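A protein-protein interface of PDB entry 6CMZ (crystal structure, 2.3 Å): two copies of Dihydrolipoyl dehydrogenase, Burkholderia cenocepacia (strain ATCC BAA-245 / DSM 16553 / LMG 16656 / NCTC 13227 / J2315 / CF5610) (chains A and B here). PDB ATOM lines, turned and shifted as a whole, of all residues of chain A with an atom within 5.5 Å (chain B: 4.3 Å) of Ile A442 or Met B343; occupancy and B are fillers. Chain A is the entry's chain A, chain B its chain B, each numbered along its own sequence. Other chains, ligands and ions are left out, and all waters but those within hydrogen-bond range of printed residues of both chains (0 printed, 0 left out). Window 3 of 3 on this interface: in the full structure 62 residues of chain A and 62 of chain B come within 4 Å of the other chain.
O of Ile A442 lies within hydrogen-bond range of OG of Ser B426 (2.8 Å).
The backbone carbonyl oxygen (O) of Pro B348 sits at hydrogen-bond distance from a ring nitrogen (NE2) of His B322, 2.5 Å away. O of Thr A441 sits close to OE1 of Gln A453 (3.4 Å). ND1 of His A443 lies within hydrogen-bond range of OE1 of Gln A453, at 3.2 Å. The backbone carbonyl oxygen of Thr A441 lies within hydrogen-bond range of a ring nitrogen (ND1) of His A443, 2.9 Å away.
Among the printed residues, merely in contact across the chains: Thr A441 with Ser B426, Ile A442 with His B322, Ile A442 with Ala B326, Ile A442 with Met B343, Ile A442 with Pro B344, Ile A442 with Pro B348, His A443 with His B322, Ala A444 with His B322 and Ala A444 with Pro B348.
Ile A442 touches just these residues of chain B: His B322, Ala B326, Met B343, Pro B344, Pro B348 and Ser B426. Printed residues of chain A within 4 Å of Met B343: Ile A442 (3.97 Å). Printed residues of chain A within 4 Å of His B322: Ile A442, His A443 and Ala A444. Printed residues of chain B within 4 Å of His A443: His B322 (3.2 Å). Of the printed residues of chain B, Ala A444 touches His B322 (3.7 Å) and Pro B348 (3.8 Å). Gln A453 touches none of the printed residues of chain B. Gly A440 touches none of the printed residues of chain B. The nearest printed residue of chain B that does not touch Ile A442 is Gln B327 (6.1 Å).
Of the 6 printed residues of chain A, 4 touch a printed residue of chain B. Along chain A the printed residues that touch a printed residue of chain B span positions 441 to 444. Of the 10 printed residues of chain B, 6 touch a printed residue of chain A. Hydrophobic or aromatic side chains of chain B that line the printed part of chain A: His B322, Ala B326, Met B343, Pro B344 and Pro B348. Among the printed residues, 10 pairs touch across the chains. Among the printed residues, no Asp or Glu carboxylate lies within 4 Å of a Lys or Arg side-chain nitrogen of the other chain.
No position is printed for both chains. Of the 10 pairs that touch across the chains among the printed residues, none has its exchanged pair printed and touching as well.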
ATOM      1  N   GLY A 440      21.052  29.876  20.353  1.00  0.00           N
ATOM      2  CA  GLY A 440      19.604  30.154  20.386  1.00  0.00           C
ATOM      3  C   GLY A 440      18.746  29.134  21.128  1.00  0.00           C
ATOM      4  O   GLY A 440      17.523  29.120  20.969  1.00  0.00           O
ATOM      5  N   THR A 441      19.381  28.281  21.924  1.00  0.00           N
ATOM      6  CA  THR A 441      18.688  27.275  22.717  1.00  0.00           C
ATOM      7  C   THR A 441      18.584  27.808  24.140  1.00  0.00           C
ATOM      8  O   THR A 441      19.585  28.245  24.702  1.00  0.00           O
ATOM      9  CB  THR A 441      19.481  25.954  22.780  1.00  0.00           C
ATOM     10  OG1 THR A 441      19.622  25.398  21.467  1.00  0.00           O
ATOM     11  CG2 THR A 441      18.776  24.942  23.691  1.00  0.00           C
ATOM     12  N   ILE A 442      17.387  27.769  24.725  1.00  0.00           N
ATOM     13  CA  ILE A 442      17.198  28.256  26.094  1.00  0.00           C
ATOM     14  C   ILE A 442      17.807  27.237  27.068  1.00  0.00           C
ATOM     15  O   ILE A 442      17.620  26.023  26.918  1.00  0.00           O
ATOM     16  CB  ILE A 442      15.702  28.537  26.415  1.00  0.00           C
ATOM     17  CG1 ILE A 442      15.166  29.606  25.471  1.00  0.00           C
ATOM     18  CG2 ILE A 442      15.507  29.033  27.848  1.00  0.00           C
ATOM     19  CD1 ILE A 442      13.735  30.041  25.746  1.00  0.00           C
ATOM     20  N   HIS A 443      18.561  27.750  28.034  1.00  0.00           N
ATOM     21  CA  HIS A 443      19.196  26.937  29.058  1.00  0.00           C
ATOM     22  C   HIS A 443      18.648  27.353  30.403  1.00  0.00           C
ATOM     23  O   HIS A 443      18.584  28.543  30.703  1.00  0.00           O
ATOM     24  CB  HIS A 443      20.724  27.088  29.019  1.00  0.00           C
ATOM     25  CG  HIS A 443      21.360  26.437  27.832  1.00  0.00           C
ATOM     26  ND1 HIS A 443      21.352  27.004  26.577  1.00  0.00           N
ATOM     27  CD2 HIS A 443      22.026  25.265  27.710  1.00  0.00           C
ATOM     28  CE1 HIS A 443      21.988  26.211  25.733  1.00  0.00           C
ATOM     29  NE2 HIS A 443      22.412  25.149  26.396  1.00  0.00           N
ATOM     30  N   ALA A 444      18.267  26.368  31.213  1.00  0.00           N
ATOM     31  CA  ALA A 444      17.684  26.628  32.533  1.00  0.00           C
ATOM     32  C   ALA A 444      18.635  27.385  33.429  1.00  0.00           C
ATOM     33  O   ALA A 444      19.848  27.113  33.445  1.00  0.00           O
ATOM     34  CB  ALA A 444      17.279  25.317  33.203  1.00  0.00           C
ATOM     35  N   GLN A 453      26.086  27.820  26.333  1.00  0.00           N
ATOM     36  CA  GLN A 453      25.427  28.812  25.498  1.00  0.00           C
ATOM     37  C   GLN A 453      26.329  30.048  25.357  1.00  0.00           C
ATOM     38  O   GLN A 453      26.563  30.526  24.246  1.00  0.00           O
ATOM     39  CB  GLN A 453      24.053  29.206  26.070  1.00  0.00           C
ATOM     40  CG  GLN A 453      23.254  30.129  25.148  1.00  0.00           C
ATOM     41  CD  GLN A 453      21.892  30.529  25.678  1.00  0.00           C
ATOM     42  OE1 GLN A 453      21.505  30.167  26.783  1.00  0.00           O
ATOM     43  NE2 GLN A 453      21.158  31.288  24.880  1.00  0.00           N
ATOM     44  N   HIS B 322      15.355  32.415  32.808  1.00  0.00           N
ATOM     45  CA  HIS B 322      15.797  32.126  31.418  1.00  0.00           C
ATOM     46  C   HIS B 322      14.727  32.442  30.373  1.00  0.00           C
ATOM     47  O   HIS B 322      15.035  32.877  29.264  1.00  0.00           O
ATOM     48  CB  HIS B 322      16.320  30.687  31.280  1.00  0.00           C
ATOM     49  CG  HIS B 322      15.414  29.636  31.867  1.00  0.00           C
ATOM     50  ND1 HIS B 322      15.322  29.411  33.225  1.00  0.00           N
ATOM     51  CD2 HIS B 322      14.614  28.714  31.281  1.00  0.00           C
ATOM     52  CE1 HIS B 322      14.482  28.417  33.452  1.00  0.00           C
ATOM     53  NE2 HIS B 322      14.045  27.972  32.288  1.00  0.00           N
ATOM     54  N   ALA B 326      15.361  35.145  27.500  1.00  0.00           N
ATOM     55  CA  ALA B 326      15.115  34.778  26.110  1.00  0.00           C
ATOM     56  C   ALA B 326      14.078  35.728  25.484  1.00  0.00           C
ATOM     57  O   ALA B 326      14.253  36.158  24.347  1.00  0.00           O
ATOM     58  CB  ALA B 326      14.659  33.332  26.002  1.00  0.00           C
ATOM     59  N   GLN B 327      13.013  36.062  26.226  1.00  0.00           N
ATOM     60  CA  GLN B 327      12.011  37.005  25.707  1.00  0.00           C
ATOM     61  C   GLN B 327      12.643  38.392  25.429  1.00  0.00           C
ATOM     62  O   GLN B 327      12.390  38.995  24.389  1.00  0.00           O
ATOM     63  CB  GLN B 327      10.821  37.172  26.660  1.00  0.00           C
ATOM     64  CG  GLN B 327       9.782  36.047  26.684  1.00  0.00           C
ATOM     65  CD  GLN B 327       8.671  36.318  27.709  1.00  0.00           C
ATOM     66  OE1 GLN B 327       8.939  36.720  28.836  1.00  0.00           O
ATOM     67  NE2 GLN B 327       7.432  36.086  27.321  1.00  0.00           N
ATOM     68  N   MET B 330      14.689  38.513  22.275  1.00  0.00           N
ATOM     69  CA  MET B 330      13.817  38.516  21.103  1.00  0.00           C
ATOM     70  C   MET B 330      13.272  39.912  20.772  1.00  0.00           C
ATOM     71  O   MET B 330      13.138  40.261  19.599  1.00  0.00           O
ATOM     72  CB  MET B 330      12.664  37.529  21.305  1.00  0.00           C
ATOM     73  CG  MET B 330      11.630  37.524  20.193  1.00  0.00           C
ATOM     74  SD  MET B 330      10.429  36.213  20.418  1.00  0.00           S
ATOM     75  CE  MET B 330       9.709  36.726  21.976  1.00  0.00           C
ATOM     76  N   PHE B 342      11.700  33.534  16.999  1.00  0.00           N
ATOM     77  CA  PHE B 342      10.588  32.820  17.658  1.00  0.00           C
ATOM     78  C   PHE B 342      11.020  32.199  18.980  1.00  0.00           C
ATOM     79  O   PHE B 342      12.179  31.824  19.137  1.00  0.00           O
ATOM     80  CB  PHE B 342      10.108  31.643  16.785  1.00  0.00           C
ATOM     81  CG  PHE B 342       9.690  32.028  15.392  1.00  0.00           C
ATOM     82  CD1 PHE B 342      10.640  32.164  14.377  1.00  0.00           C
ATOM     83  CD2 PHE B 342       8.342  32.211  15.076  1.00  0.00           C
ATOM     84  CE1 PHE B 342      10.257  32.510  13.088  1.00  0.00           C
ATOM     85  CE2 PHE B 342       7.953  32.549  13.787  1.00  0.00           C
ATOM     86  CZ  PHE B 342       8.911  32.700  12.791  1.00  0.00           C
ATOM     87  N   MET B 343      10.079  32.065  19.912  1.00  0.00           N
ATOM     88  CA  MET B 343      10.352  31.414  21.193  1.00  0.00           C
ATOM     89  C   MET B 343      10.309  29.904  20.961  1.00  0.00           C
ATOM     90  O   MET B 343       9.442  29.421  20.227  1.00  0.00           O
ATOM     91  CB  MET B 343       9.327  31.814  22.246  1.00  0.00           C
ATOM     92  CG  MET B 343       9.493  33.227  22.774  1.00  0.00           C
ATOM     93  SD  MET B 343      10.965  33.412  23.797  1.00  0.00           S
ATOM     94  CE  MET B 343      10.569  32.369  25.206  1.00  0.00           C
ATOM     95  N   PRO B 344      11.228  29.149  21.599  1.00  0.00           N
ATOM     96  CA  PRO B 344      11.276  27.699  21.371  1.00  0.00           C
ATOM     97  C   PRO B 344      10.025  26.955  21.799  1.00  0.00           C
ATOM     98  O   PRO B 344       9.304  27.391  22.705  1.00  0.00           O
ATOM     99  CB  PRO B 344      12.462  27.248  22.227  1.00  0.00           C
ATOM    100  CG  PRO B 344      12.491  28.224  23.337  1.00  0.00           C
ATOM    101  CD  PRO B 344      12.126  29.543  22.701  1.00  0.00           C
ATOM    102  N   ALA B 345       9.797  25.822  21.141  1.00  0.00           N
ATOM    103  CA  ALA B 345       8.649  24.971  21.416  1.00  0.00           C
ATOM    104  C   ALA B 345       8.647  24.444  22.862  1.00  0.00           C
ATOM    105  O   ALA B 345       7.581  24.137  23.395  1.00  0.00           O
ATOM    106  CB  ALA B 345       8.611  23.811  20.421  1.00  0.00           C
ATOM    107  N   PRO B 348      12.985  24.599  29.349  1.00  0.00           N
ATOM    108  CA  PRO B 348      13.353  23.711  30.437  1.00  0.00           C
ATOM    109  C   PRO B 348      13.203  24.361  31.803  1.00  0.00           C
ATOM    110  O   PRO B 348      13.214  25.593  31.923  1.00  0.00           O
ATOM    111  CB  PRO B 348      14.831  23.439  30.172  1.00  0.00           C
ATOM    112  CG  PRO B 348      15.318  24.698  29.547  1.00  0.00           C
ATOM    113  CD  PRO B 348      14.171  25.224  28.736  1.00  0.00           C
ATOM    114  N   SER B 426      16.967  20.487  26.688  1.00  0.00           N
ATOM    115  CA  SER B 426      16.592  21.611  25.791  1.00  0.00           C
ATOM    116  C   SER B 426      17.321  21.639  24.434  1.00  0.00           C
ATOM    117  O   SER B 426      16.717  22.004  23.416  1.00  0.00           O
ATOM    118  CB  SER B 426      16.686  22.969  26.478  1.00  0.00           C
ATOM    119  OG  SER B 426      17.973  23.200  26.943  1.00  0.00           O
